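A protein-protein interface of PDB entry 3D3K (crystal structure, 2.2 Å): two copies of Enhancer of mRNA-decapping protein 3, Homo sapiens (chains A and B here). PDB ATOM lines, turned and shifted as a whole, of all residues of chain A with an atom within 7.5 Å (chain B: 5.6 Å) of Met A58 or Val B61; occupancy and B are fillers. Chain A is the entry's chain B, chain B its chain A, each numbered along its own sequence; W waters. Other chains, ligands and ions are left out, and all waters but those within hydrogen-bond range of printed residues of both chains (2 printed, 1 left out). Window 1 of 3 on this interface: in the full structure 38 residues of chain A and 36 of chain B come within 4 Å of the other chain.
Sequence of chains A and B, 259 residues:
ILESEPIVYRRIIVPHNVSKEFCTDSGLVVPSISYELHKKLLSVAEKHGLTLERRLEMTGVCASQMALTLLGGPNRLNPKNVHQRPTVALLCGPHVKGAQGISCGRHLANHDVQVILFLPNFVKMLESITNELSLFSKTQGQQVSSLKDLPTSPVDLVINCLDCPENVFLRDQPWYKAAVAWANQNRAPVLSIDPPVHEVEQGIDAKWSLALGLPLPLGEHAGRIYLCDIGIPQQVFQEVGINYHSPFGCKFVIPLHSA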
ATOM      1  N   LEU A  50      -5.136  -6.075 -17.770  1.00  0.00           N
ATOM      2  CA  LEU A  50      -3.972  -5.202 -17.748  1.00  0.00           C
ATOM      3  C   LEU A  50      -3.520  -5.067 -16.309  1.00  0.00           C
ATOM      4  O   LEU A  50      -3.783  -4.058 -15.635  1.00  0.00           O
ATOM      5  CB  LEU A  50      -4.274  -3.850 -18.377  1.00  0.00           C
ATOM      6  CG  LEU A  50      -3.015  -3.067 -18.756  1.00  0.00           C
ATOM      7  CD1 LEU A  50      -2.332  -3.695 -19.979  1.00  0.00           C
ATOM      8  CD2 LEU A  50      -3.352  -1.628 -19.001  1.00  0.00           C
ATOM      9  N   LEU A  52      -1.228  -4.983 -12.797  1.00  0.00           N
ATOM     10  CA  LEU A  52      -0.226  -4.058 -12.294  1.00  0.00           C
ATOM     11  C   LEU A  52       1.185  -4.467 -12.734  1.00  0.00           C
ATOM     12  O   LEU A  52       1.950  -3.637 -13.201  1.00  0.00           O
ATOM     13  CB  LEU A  52      -0.312  -3.944 -10.757  1.00  0.00           C
ATOM     14  CG  LEU A  52       0.720  -3.015 -10.093  1.00  0.00           C
ATOM     15  CD1 LEU A  52       0.626  -1.595 -10.659  1.00  0.00           C
ATOM     16  CD2 LEU A  52       0.580  -3.007  -8.554  1.00  0.00           C
ATOM     17  N   GLU A  53       1.515  -5.749 -12.585  1.00  0.00           N
ATOM     18  CA  GLU A  53       2.819  -6.258 -13.006  1.00  0.00           C
ATOM     19  C   GLU A  53       3.131  -5.981 -14.481  1.00  0.00           C
ATOM     20  O   GLU A  53       4.247  -5.583 -14.803  1.00  0.00           O
ATOM     21  CB  GLU A  53       2.995  -7.742 -12.645  1.00  0.00           C
ATOM     22  CG  GLU A  53       3.139  -7.967 -11.126  1.00  0.00           C
ATOM     23  CD  GLU A  53       4.016  -9.161 -10.748  1.00  0.00           C
ATOM     24  OE1 GLU A  53       5.210  -9.202 -11.147  1.00  0.00           O
ATOM     25  OE2 GLU A  53       3.496 -10.060 -10.022  1.00  0.00           O
ATOM     26  N   ARG A  54       2.140  -6.160 -15.358  1.00  0.00           N
ATOM     27  CA  ARG A  54       2.296  -5.800 -16.770  1.00  0.00           C
ATOM     28  C   ARG A  54       2.606  -4.304 -16.952  1.00  0.00           C
ATOM     29  O   ARG A  54       3.513  -3.930 -17.706  1.00  0.00           O
ATOM     30  CB  ARG A  54       1.046  -6.192 -17.580  1.00  0.00           C
ATOM     31  CG  ARG A  54       0.864  -7.687 -17.810  1.00  0.00           C
ATOM     32  CD  ARG A  54      -0.411  -7.957 -18.634  1.00  0.00           C
ATOM     33  NE  ARG A  54      -0.501  -9.335 -19.112  1.00  0.00           N
ATOM     34  CZ  ARG A  54      -0.178  -9.741 -20.336  1.00  0.00           C
ATOM     35  NH1 ARG A  54      -0.311 -11.025 -20.664  1.00  0.00           N
ATOM     36  NH2 ARG A  54       0.284  -8.873 -21.237  1.00  0.00           N
ATOM     37  N   ARG A  55       1.846  -3.452 -16.255  1.00  0.00           N
ATOM     38  CA  ARG A  55       2.021  -1.994 -16.345  1.00  0.00           C
ATOM     39  C   ARG A  55       3.339  -1.507 -15.740  1.00  0.00           C
ATOM     40  O   ARG A  55       3.964  -0.582 -16.268  1.00  0.00           O
ATOM     41  CB  ARG A  55       0.832  -1.252 -15.715  1.00  0.00           C
ATOM     42  CG  ARG A  55      -0.456  -1.458 -16.504  1.00  0.00           C
ATOM     43  CD  ARG A  55      -1.633  -0.607 -16.032  1.00  0.00           C
ATOM     44  NE  ARG A  55      -1.606  -0.296 -14.606  1.00  0.00           N
ATOM     45  CZ  ARG A  55      -2.184  -1.011 -13.642  1.00  0.00           C
ATOM     46  NH1 ARG A  55      -2.846  -2.125 -13.904  1.00  0.00           N
ATOM     47  NH2 ARG A  55      -2.088  -0.592 -12.398  1.00  0.00           N
ATOM     48  N   LEU A  56       3.755  -2.118 -14.637  1.00  0.00           N
ATOM     49  CA  LEU A  56       5.072  -1.828 -14.053  1.00  0.00           C
ATOM     50  C   LEU A  56       6.208  -2.101 -15.056  1.00  0.00           C
ATOM     51  O   LEU A  56       7.110  -1.271 -15.221  1.00  0.00           O
ATOM     52  CB  LEU A  56       5.288  -2.626 -12.765  1.00  0.00           C
ATOM     53  CG  LEU A  56       4.471  -2.233 -11.536  1.00  0.00           C
ATOM     54  CD1 LEU A  56       4.657  -3.243 -10.381  1.00  0.00           C
ATOM     55  CD2 LEU A  56       4.821  -0.819 -11.086  1.00  0.00           C
ATOM     56  N   GLU A  57       6.150  -3.255 -15.723  1.00  0.00           N
ATOM     57  CA  GLU A  57       7.130  -3.607 -16.742  1.00  0.00           C
ATOM     58  C   GLU A  57       7.091  -2.621 -17.917  1.00  0.00           C
ATOM     59  O   GLU A  57       8.132  -2.126 -18.346  1.00  0.00           O
ATOM     60  CB  GLU A  57       6.902  -5.034 -17.241  1.00  0.00           C
ATOM     61  CG  GLU A  57       8.045  -5.624 -18.079  1.00  0.00           C
ATOM     62  CD  GLU A  57       9.319  -5.895 -17.263  1.00  0.00           C
ATOM     63  OE1 GLU A  57       9.229  -6.079 -16.025  1.00  0.00           O
ATOM     64  OE2 GLU A  57      10.418  -5.933 -17.866  1.00  0.00           O
ATOM     65  N   MET A  58       5.893  -2.330 -18.420  1.00  0.00           N
ATOM     66  CA  MET A  58       5.748  -1.439 -19.567  1.00  0.00           C
ATOM     67  C   MET A  58       6.210  -0.038 -19.214  1.00  0.00           C
ATOM     68  O   MET A  58       6.936   0.583 -19.976  1.00  0.00           O
ATOM     69  CB  MET A  58       4.300  -1.417 -20.092  1.00  0.00           C
ATOM     70  CG  MET A  58       4.019  -0.313 -21.121  1.00  0.00           C
ATOM     71  SD  MET A  58       2.565  -0.583 -22.154  1.00  0.00           S
ATOM     72  CE  MET A  58       2.819   0.612 -23.455  1.00  0.00           C
ATOM     73  N   THR A  59       5.763   0.457 -18.062  1.00  0.00           N
ATOM     74  CA  THR A  59       6.142   1.788 -17.596  1.00  0.00           C
ATOM     75  C   THR A  59       7.663   1.909 -17.475  1.00  0.00           C
ATOM     76  O   THR A  59       8.245   2.907 -17.918  1.00  0.00           O
ATOM     77  CB  THR A  59       5.427   2.143 -16.259  1.00  0.00           C
ATOM     78  OG1 THR A  59       4.013   2.042 -16.456  1.00  0.00           O
ATOM     79  CG2 THR A  59       5.761   3.564 -15.802  1.00  0.00           C
ATOM     80  N   GLY A  60       8.295   0.888 -16.902  1.00  0.00           N
ATOM     81  CA  GLY A  60       9.753   0.835 -16.778  1.00  0.00           C
ATOM     82  C   GLY A  60      10.472   0.902 -18.121  1.00  0.00           C
ATOM     83  O   GLY A  60      11.453   1.627 -18.270  1.00  0.00           O
ATOM     84  N   VAL A  61       9.966   0.160 -19.102  1.00  0.00           N
ATOM     85  CA  VAL A  61      10.526   0.167 -20.445  1.00  0.00           C
ATOM     86  C   VAL A  61      10.454   1.563 -21.083  1.00  0.00           C
ATOM     87  O   VAL A  61      11.483   2.115 -21.505  1.00  0.00           O
ATOM     88  CB  VAL A  61       9.835  -0.878 -21.368  1.00  0.00           C
ATOM     89  CG1 VAL A  61      10.210  -0.647 -22.838  1.00  0.00           C
ATOM     90  CG2 VAL A  61      10.186  -2.290 -20.933  1.00  0.00           C
ATOM     91  N   CYS A  62       9.244   2.120 -21.135  1.00  0.00           N
ATOM     92  CA  CYS A  62       8.997   3.385 -21.822  1.00  0.00           C
ATOM     93  C   CYS A  62       9.601   4.585 -21.108  1.00  0.00           C
ATOM     94  O   CYS A  62      10.059   5.532 -21.758  1.00  0.00           O
ATOM     95  CB  CYS A  62       7.501   3.602 -22.041  1.00  0.00           C
ATOM     96  SG  CYS A  62       6.740   2.389 -23.122  1.00  0.00           S
ATOM     97  N   ALA A  63       9.590   4.555 -19.780  1.00  0.00           N
ATOM     98  CA  ALA A  63      10.264   5.591 -18.997  1.00  0.00           C
ATOM     99  C   ALA A  63      11.783   5.528 -19.175  1.00  0.00           C
ATOM    100  O   ALA A  63      12.431   6.560 -19.302  1.00  0.00           O
ATOM    101  CB  ALA A  63       9.883   5.508 -17.519  1.00  0.00           C
ATOM    102  N   SER A  64      12.341   4.319 -19.210  1.00  0.00           N
ATOM    103  CA  SER A  64      13.780   4.156 -19.405  1.00  0.00           C
ATOM    104  C   SER A  64      14.194   4.623 -20.797  1.00  0.00           C
ATOM    105  O   SER A  64      15.257   5.216 -20.956  1.00  0.00           O
ATOM    106  CB  SER A  64      14.246   2.720 -19.107  1.00  0.00           C
ATOM    107  OG  SER A  64      13.870   1.797 -20.122  1.00  0.00           O
ATOM    108  N   GLN A  65      13.331   4.391 -21.785  1.00  0.00           N
ATOM    109  CA  GLN A  65      13.530   4.876 -23.159  1.00  0.00           C
ATOM    110  C   GLN A  65      13.548   6.394 -23.188  1.00  0.00           C
ATOM    111  O   GLN A  65      14.405   6.989 -23.836  1.00  0.00           O
ATOM    112  CB  GLN A  65      12.439   4.352 -24.100  1.00  0.00           C
ATOM    113  CG  GLN A  65      12.600   2.869 -24.458  1.00  0.00           C
ATOM    114  CD  GLN A  65      11.531   2.332 -25.408  1.00  0.00           C
ATOM    115  OE1 GLN A  65      10.403   2.808 -25.441  1.00  0.00           O
ATOM    116  NE2 GLN A  65      11.888   1.310 -26.164  1.00  0.00           N
ATOM    117  N   SER A 103      11.524  -0.332 -11.564  1.00  0.00           N
ATOM    118  CA  SER A 103      11.376  -0.903 -12.904  1.00  0.00           C
ATOM    119  C   SER A 103      12.161  -0.121 -13.949  1.00  0.00           C
ATOM    120  O   SER A 103      12.924  -0.705 -14.705  1.00  0.00           O
ATOM    121  CB  SER A 103       9.909  -0.953 -13.318  1.00  0.00           C
ATOM    122  OG  SER A 103       9.791  -1.645 -14.549  1.00  0.00           O
ATOM    123  N   ARG A 106      15.893  -0.739 -13.292  1.00  0.00           N
ATOM    124  CA  ARG A 106      16.409  -2.026 -13.784  1.00  0.00           C
ATOM    125  C   ARG A 106      16.648  -1.996 -15.300  1.00  0.00           C
ATOM    126  O   ARG A 106      17.673  -2.483 -15.783  1.00  0.00           O
ATOM    127  CB  ARG A 106      15.494  -3.199 -13.416  1.00  0.00           C
ATOM    128  CG  ARG A 106      15.692  -4.404 -14.347  1.00  0.00           C
ATOM    129  CD  ARG A 106      14.724  -5.549 -14.159  1.00  0.00           C
ATOM    130  NE  ARG A 106      13.328  -5.156 -13.992  1.00  0.00           N
ATOM    131  CZ  ARG A 106      12.351  -5.433 -14.851  1.00  0.00           C
ATOM    132  NH1 ARG A 106      12.601  -6.088 -15.985  1.00  0.00           N
ATOM    133  NH2 ARG A 106      11.119  -5.040 -14.572  1.00  0.00           N
ATOM    134  N   HIS A 107      15.702  -1.425 -16.043  1.00  0.00           N
ATOM    135  CA  HIS A 107      15.829  -1.319 -17.497  1.00  0.00           C
ATOM    136  C   HIS A 107      16.993  -0.432 -17.903  1.00  0.00           C
ATOM    137  O   HIS A 107      17.690  -0.752 -18.848  1.00  0.00           O
ATOM    138  CB  HIS A 107      14.532  -0.833 -18.143  1.00  0.00           C
ATOM    139  CG  HIS A 107      13.441  -1.852 -18.119  1.00  0.00           C
ATOM    140  ND1 HIS A 107      13.471  -2.990 -18.900  1.00  0.00           N
ATOM    141  CD2 HIS A 107      12.298  -1.918 -17.395  1.00  0.00           C
ATOM    142  CE1 HIS A 107      12.387  -3.705 -18.666  1.00  0.00           C
ATOM    143  NE2 HIS A 107      11.660  -3.079 -17.757  1.00  0.00           N
ATOM    144  N   GLU A 132      10.032  -5.908  -7.914  1.00  0.00           N
ATOM    145  CA  GLU A 132      10.923  -5.027  -8.665  1.00  0.00           C
ATOM    146  C   GLU A 132      12.361  -5.054  -8.144  1.00  0.00           C
ATOM    147  O   GLU A 132      13.311  -5.090  -8.939  1.00  0.00           O
ATOM    148  CB  GLU A 132      10.377  -3.596  -8.734  1.00  0.00           C
ATOM    149  CG  GLU A 132       9.115  -3.414  -9.617  1.00  0.00           C
ATOM    150  CD  GLU A 132       9.304  -3.725 -11.108  1.00  0.00           C
ATOM    151  OE1 GLU A 132      10.438  -3.948 -11.596  1.00  0.00           O
ATOM    152  OE2 GLU A 132       8.277  -3.739 -11.808  1.00  0.00           O
ATOM    153  N   CYS A 228       2.995   9.025 -21.314  1.00  0.00           N
ATOM    154  CA  CYS A 228       3.443   7.680 -21.585  1.00  0.00           C
ATOM    155  C   CYS A 228       2.240   6.802 -21.880  1.00  0.00           C
ATOM    156  O   CYS A 228       1.246   6.841 -21.166  1.00  0.00           O
ATOM    157  CB  CYS A 228       4.219   7.136 -20.370  1.00  0.00           C
ATOM    158  SG  CYS A 228       5.059   5.560 -20.636  1.00  0.00           S
ATOM    159  N   ASP A 229       2.339   6.024 -22.955  1.00  0.00           N
ATOM    160  CA  ASP A 229       1.382   4.967 -23.227  1.00  0.00           C
ATOM    161  C   ASP A 229       1.635   3.833 -22.228  1.00  0.00           C
ATOM    162  O   ASP A 229       2.764   3.356 -22.086  1.00  0.00           O
ATOM    163  CB  ASP A 229       1.548   4.482 -24.674  1.00  0.00           C
ATOM    164  CG  ASP A 229       0.544   3.427 -25.065  1.00  0.00           C
ATOM    165  OD1 ASP A 229      -0.473   3.231 -24.350  1.00  0.00           O
ATOM    166  OD2 ASP A 229       0.774   2.776 -26.108  1.00  0.00           O
ATOM    167  N   ILE A 230       0.593   3.423 -21.512  1.00  0.00           N
ATOM    168  CA  ILE A 230       0.714   2.287 -20.587  1.00  0.00           C
ATOM    169  C   ILE A 230      -0.100   1.055 -21.019  1.00  0.00           C
ATOM    170  O   ILE A 230      -0.293   0.118 -20.236  1.00  0.00           O
ATOM    171  CB  ILE A 230       0.480   2.680 -19.093  1.00  0.00           C
ATOM    172  CG1 ILE A 230      -0.873   3.369 -18.901  1.00  0.00           C
ATOM    173  CG2 ILE A 230       1.642   3.552 -18.573  1.00  0.00           C
ATOM    174  CD1 ILE A 230      -1.296   3.483 -17.450  1.00  0.00           C
ATOM    175  N   GLY A 231      -0.570   1.070 -22.268  1.00  0.00           N
ATOM    176  CA  GLY A 231      -1.101  -0.121 -22.931  1.00  0.00           C
ATOM    177  C   GLY A 231      -2.603  -0.300 -22.864  1.00  0.00           C
ATOM    178  O   GLY A 231      -3.118  -1.406 -23.118  1.00  0.00           O
ATOM    179  N   ILE A 232      -3.301   0.791 -22.542  1.00  0.00           N
ATOM    180  CA  ILE A 232      -4.748   0.779 -22.297  1.00  0.00           C
ATOM    181  C   ILE A 232      -5.526   0.817 -23.607  1.00  0.00           C
ATOM    182  O   ILE A 232      -5.413   1.788 -24.368  1.00  0.00           O
ATOM    183  CB  ILE A 232      -5.189   1.969 -21.411  1.00  0.00           C
ATOM    184  CG1 ILE A 232      -4.465   1.937 -20.064  1.00  0.00           C
ATOM    185  CG2 ILE A 232      -6.697   1.940 -21.180  1.00  0.00           C
ATOM    186  CD1 ILE A 232      -4.664   3.195 -19.230  1.00  0.00           C
ATOM    187  N   PHE A 252       5.501   6.122 -28.048  1.00  0.00           N
ATOM    188  CA  PHE A 252       4.977   5.616 -26.779  1.00  0.00           C
ATOM    189  C   PHE A 252       5.148   6.646 -25.659  1.00  0.00           C
ATOM    190  O   PHE A 252       4.503   6.541 -24.610  1.00  0.00           O
ATOM    191  CB  PHE A 252       5.661   4.291 -26.404  1.00  0.00           C
ATOM    192  CG  PHE A 252       5.085   3.091 -27.106  1.00  0.00           C
ATOM    193  CD1 PHE A 252       4.327   2.155 -26.400  1.00  0.00           C
ATOM    194  CD2 PHE A 252       5.283   2.900 -28.480  1.00  0.00           C
ATOM    195  CE1 PHE A 252       3.785   1.032 -27.047  1.00  0.00           C
ATOM    196  CE2 PHE A 252       4.748   1.796 -29.139  1.00  0.00           C
ATOM    197  CZ  PHE A 252       3.996   0.853 -28.417  1.00  0.00           C
ATOM    198  N   LEU B  56       5.549 -10.940 -21.821  1.00  0.00           N
ATOM    199  CA  LEU B  56       4.544 -10.792 -22.880  1.00  0.00           C
ATOM    200  C   LEU B  56       4.217  -9.331 -23.123  1.00  0.00           C
ATOM    201  O   LEU B  56       4.080  -8.895 -24.270  1.00  0.00           O
ATOM    202  CB  LEU B  56       3.258 -11.563 -22.533  1.00  0.00           C
ATOM    203  CG  LEU B  56       3.325 -13.086 -22.618  1.00  0.00           C
ATOM    204  CD1 LEU B  56       2.032 -13.726 -22.099  1.00  0.00           C
ATOM    205  CD2 LEU B  56       3.623 -13.533 -24.057  1.00  0.00           C
ATOM    206  N   GLU B  57       4.095  -8.571 -22.042  1.00  0.00           N
ATOM    207  CA  GLU B  57       3.818  -7.147 -22.158  1.00  0.00           C
ATOM    208  C   GLU B  57       4.972  -6.402 -22.824  1.00  0.00           C
ATOM    209  O   GLU B  57       4.741  -5.613 -23.751  1.00  0.00           O
ATOM    210  CB  GLU B  57       3.477  -6.528 -20.798  1.00  0.00           C
ATOM    211  CG  GLU B  57       2.874  -5.119 -20.868  1.00  0.00           C
ATOM    212  CD  GLU B  57       1.459  -5.104 -21.479  1.00  0.00           C
ATOM    213  OE1 GLU B  57       0.802  -6.170 -21.519  1.00  0.00           O
ATOM    214  OE2 GLU B  57       1.007  -4.018 -21.909  1.00  0.00           O
ATOM    215  N   MET B  58       6.200  -6.662 -22.362  1.00  0.00           N
ATOM    216  CA  MET B  58       7.401  -5.972 -22.888  1.00  0.00           C
ATOM    217  C   MET B  58       7.702  -6.357 -24.331  1.00  0.00           C
ATOM    218  O   MET B  58       8.137  -5.526 -25.136  1.00  0.00           O
ATOM    219  CB  MET B  58       8.617  -6.234 -21.983  1.00  0.00           C
ATOM    220  CG  MET B  58       9.984  -5.928 -22.594  1.00  0.00           C
ATOM    221  SD  MET B  58      11.291  -5.819 -21.344  1.00  0.00           S
ATOM    222  CE  MET B  58      12.535  -4.866 -22.213  1.00  0.00           C
ATOM    223  N   THR B  59       7.482  -7.630 -24.641  1.00  0.00           N
ATOM    224  CA  THR B  59       7.717  -8.157 -25.979  1.00  0.00           C
ATOM    225  C   THR B  59       6.746  -7.517 -26.966  1.00  0.00           C
ATOM    226  O   THR B  59       7.138  -7.163 -28.077  1.00  0.00           O
ATOM    227  CB  THR B  59       7.650  -9.693 -25.971  1.00  0.00           C
ATOM    228  OG1 THR B  59       8.597 -10.174 -25.011  1.00  0.00           O
ATOM    229  CG2 THR B  59       8.001 -10.284 -27.325  1.00  0.00           C
ATOM    230  N   GLY B  60       5.501  -7.325 -26.542  1.00  0.00           N
ATOM    231  CA  GLY B  60       4.499  -6.677 -27.377  1.00  0.00           C
ATOM    232  C   GLY B  60       4.816  -5.214 -27.655  1.00  0.00           C
ATOM    233  O   GLY B  60       4.653  -4.753 -28.781  1.00  0.00           O
ATOM    234  N   VAL B  61       5.269  -4.496 -26.627  1.00  0.00           N
ATOM    235  CA  VAL B  61       5.662  -3.096 -26.756  1.00  0.00           C
ATOM    236  C   VAL B  61       6.852  -2.957 -27.704  1.00  0.00           C
ATOM    237  O   VAL B  61       6.807  -2.185 -28.651  1.00  0.00           O
ATOM    238  CB  VAL B  61       6.007  -2.457 -25.377  1.00  0.00           C
ATOM    239  CG1 VAL B  61       6.534  -1.045 -25.543  1.00  0.00           C
ATOM    240  CG2 VAL B  61       4.794  -2.468 -24.459  1.00  0.00           C
ATOM    241  N   CYS B  62       7.904  -3.721 -27.431  1.00  0.00           N
ATOM    242  CA  CYS B  62       9.138  -3.652 -28.198  1.00  0.00           C
ATOM    243  C   CYS B  62       8.972  -4.200 -29.618  1.00  0.00           C
ATOM    244  O   CYS B  62       9.538  -3.644 -30.563  1.00  0.00           O
ATOM    245  CB  CYS B  62      10.278  -4.348 -27.438  1.00  0.00           C
ATOM    246  SG  CYS B  62      10.764  -3.450 -25.920  1.00  0.00           S
ATOM    247  N   ALA B  63       8.173  -5.256 -29.784  1.00  0.00           N
ATOM    248  CA  ALA B  63       7.891  -5.746 -31.137  1.00  0.00           C
ATOM    249  C   ALA B  63       7.054  -4.750 -31.942  1.00  0.00           C
ATOM    250  O   ALA B  63       7.290  -4.562 -33.137  1.00  0.00           O
ATOM    251  CB  ALA B  63       7.237  -7.118 -31.110  1.00  0.00           C
ATOM    252  N   SER B  64       6.088  -4.106 -31.289  1.00  0.00           N
ATOM    253  CA  SER B  64       5.207  -3.157 -31.968  1.00  0.00           C
ATOM    254  C   SER B  64       5.966  -1.909 -32.368  1.00  0.00           C
ATOM    255  O   SER B  64       5.688  -1.326 -33.410  1.00  0.00           O
ATOM    256  CB  SER B  64       3.982  -2.807 -31.112  1.00  0.00           C
ATOM    257  OG  SER B  64       4.349  -2.015 -29.994  1.00  0.00           O
ATOM    258  N   GLN B  65       6.938  -1.517 -31.544  1.00  0.00           N
ATOM    259  CA  GLN B  65       7.848  -0.417 -31.864  1.00  0.00           C
ATOM    260  C   GLN B  65       8.657  -0.741 -33.115  1.00  0.00           C
ATOM    261  O   GLN B  65       8.807   0.110 -33.992  1.00  0.00           O
ATOM    262  CB  GLN B  65       8.779  -0.099 -30.689  1.00  0.00           C
ATOM    263  CG  GLN B  65       8.078   0.625 -29.518  1.00  0.00           C
ATOM    264  CD  GLN B  65       8.988   0.867 -28.316  1.00  0.00           C
ATOM    265  OE1 GLN B  65      10.001   0.188 -28.134  1.00  0.00           O
ATOM    266  NE2 GLN B  65       8.616   1.839 -27.483  1.00  0.00           N
ATOM    267  N   MET B  66       9.165  -1.967 -33.198  1.00  0.00           N
ATOM    268  CA  MET B  66       9.854  -2.432 -34.399  1.00  0.00           C
ATOM    269  C   MET B  66       8.922  -2.365 -35.607  1.00  0.00           C
ATOM    270  O   MET B  66       9.285  -1.809 -36.629  1.00  0.00           O
ATOM    271  CB  MET B  66      10.382  -3.863 -34.229  1.00  0.00           C
ATOM    272  CG  MET B  66      11.114  -4.378 -35.472  1.00  0.00           C
ATOM    273  SD  MET B  66      11.612  -6.098 -35.398  1.00  0.00           S
ATOM    274  CE  MET B  66      12.319  -6.281 -37.026  1.00  0.00           C
ATOM    275  N   SER B 103      -0.234  -9.703 -28.062  1.00  0.00           N
ATOM    276  CA  SER B 103       0.299  -8.550 -27.348  1.00  0.00           C
ATOM    277  C   SER B 103       0.787  -7.485 -28.325  1.00  0.00           C
ATOM    278  O   SER B 103       0.447  -6.298 -28.198  1.00  0.00           O
ATOM    279  CB  SER B 103       1.467  -8.978 -26.450  1.00  0.00           C
ATOM    280  OG  SER B 103       1.834  -7.919 -25.586  1.00  0.00           O
ATOM    281  N   CYS B 104       1.606  -7.911 -29.285  1.00  0.00           N
ATOM    282  CA  CYS B 104       2.117  -7.003 -30.309  1.00  0.00           C
ATOM    283  C   CYS B 104       0.961  -6.350 -31.073  1.00  0.00           C
ATOM    284  O   CYS B 104       0.944  -5.139 -31.284  1.00  0.00           O
ATOM    285  CB  CYS B 104       3.066  -7.747 -31.256  1.00  0.00           C
ATOM    286  SG  CYS B 104       3.745  -6.701 -32.566  1.00  0.00           S
ATOM    287  N   HIS B 107      -0.871  -3.613 -28.957  1.00  0.00           N
ATOM    288  CA  HIS B 107      -0.077  -2.393 -28.889  1.00  0.00           C
ATOM    289  C   HIS B 107      -0.094  -1.642 -30.226  1.00  0.00           C
ATOM    290  O   HIS B 107      -0.134  -0.416 -30.238  1.00  0.00           O
ATOM    291  CB  HIS B 107       1.362  -2.670 -28.426  1.00  0.00           C
ATOM    292  CG  HIS B 107       1.464  -3.038 -26.980  1.00  0.00           C
ATOM    293  ND1 HIS B 107       1.279  -2.123 -25.963  1.00  0.00           N
ATOM    294  CD2 HIS B 107       1.719  -4.225 -26.377  1.00  0.00           C
ATOM    295  CE1 HIS B 107       1.414  -2.733 -24.799  1.00  0.00           C
ATOM    296  NE2 HIS B 107       1.676  -4.010 -25.023  1.00  0.00           N
HETATM  297  O   HOH W   1      -0.092   0.205 -26.334  1.00  0.00           O
HETATM  298  O   HOH W   2      10.198  -8.299 -19.630  1.00  0.00           O
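The side-chain carboxylate (OE1) of Glu B57 is in salt-bridge range of the guanidinium group (NH2) of Arg A54. SD of Met A58 lies close to OE2 of Glu B57 (3.8 Å). OE1 of Gln A65 lies within hydrogen-bond range of NE2 of Gln B65 (2.9 Å). The side-chain sulfur (SD) of Met B58 lies close to the side-chain carboxylate (OE2) of Glu A57 (3.6 Å).
The guanidinium group (NH1) of Arg A55 lies within hydrogen-bond range of the backbone carbonyl oxygen (O) of Leu A50. The side-chain carboxylate (OE1) of Glu A57 lies within salt-bridge range of the guanidinium group (NH2) of Arg A106 (2.6 Å). The backbone carbonyl oxygen (O) of Val B61 sits at hydrogen-bond distance from the side-chain hydroxyl (OG) of Ser B64, 2.8 Å away. N of Gly A231 lies within hydrogen-bond range of SD of Met A58 (3.5 Å). The side-chain hydroxyl (OG) of Ser B64 lies within hydrogen-bond range of the backbone carbonyl oxygen (O) of Gly B60, 3.0 Å away. OE2 of Glu A57 lies close to NE2 of His A107 (3.1 Å).
Among the printed residues, pairs that only touch across the chains: Leu A50 with Glu B57 (3.9 Å), Arg A54 with Leu B56 (3.9 Å), Met A58 with Val B61 (3.7 Å), Met A58 with His B107 (3.6 Å), Val A61 with Met B58 (3.7 Å), His A107 with Met B58 (3.6 Å), Phe A252 with Val B61 (3.8 Å), Phe A252 with Ser B64 (3.3 Å) and Phe A252 with Gln B65 (3.6 Å).
Met A58 touches just these residues of chain B: Glu B57 (3.8 Å), Val B61 (3.7 Å) and His B107 (3.6 Å). Of the printed residues of chain B, Gln A65 touches Gln B65 (2.9 Å). Of the printed residues of chain A, Glu B57 touches Leu A50 (3.9 Å), Arg A54 (2.8 Å) and Met A58 (3.8 Å). Printed residues of chain A within 4 Å of Val B61: Met A58 (3.7 Å) and Phe A252 (3.8 Å). Cys B62 touches none of the printed residues of chain A. The nearest printed residue of chain B that does not touch Met A58 is Met B58 (5.9 Å).
Of the 14 printed residues of chain B, 7 touch a printed residue of chain A. Printed residues of chain B that touch a printed residue of chain A: Leu B56, Glu B57, Met B58, Val B61, Ser B64, Gln B65 and His B107. Hydrophobic or aromatic side chains of chain B that line the printed part of chain A: Leu B56, Met B58, Val B61 and His B107. Hydrophobic or aromatic side chains of chain A within 4 Å of the printed part of chain B: Leu A50, Met A58, Val A61, His A107 and Phe A252. Among the printed residues, 13 pairs touch across the chains.
Glu A57 touches Met B58, and with the chains exchanged Met A58 touches Glu B57. Met A58 touches Val B61, and with the chains exchanged Val A61 touches Met B58. Met A58 touches His B107, and with the chains exchanged His A107 touches Met B58. Gln A65 touches its own counterpart, Gln B65. Of the 13 pairs that touch across the chains among the printed residues, 7 have their exchanged pair printed and touching as well.
Water W1 bridges the side-chain carboxylate of Asp A229 (2.7 Å) and a ring nitrogen (ND1) of His B107 (2.7 Å). Water W2 bridges the side-chain carboxylate (OE2) of Glu A57 (3.0 Å) and the side-chain sulfur (SD) of Met B58 (3.2 Å).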
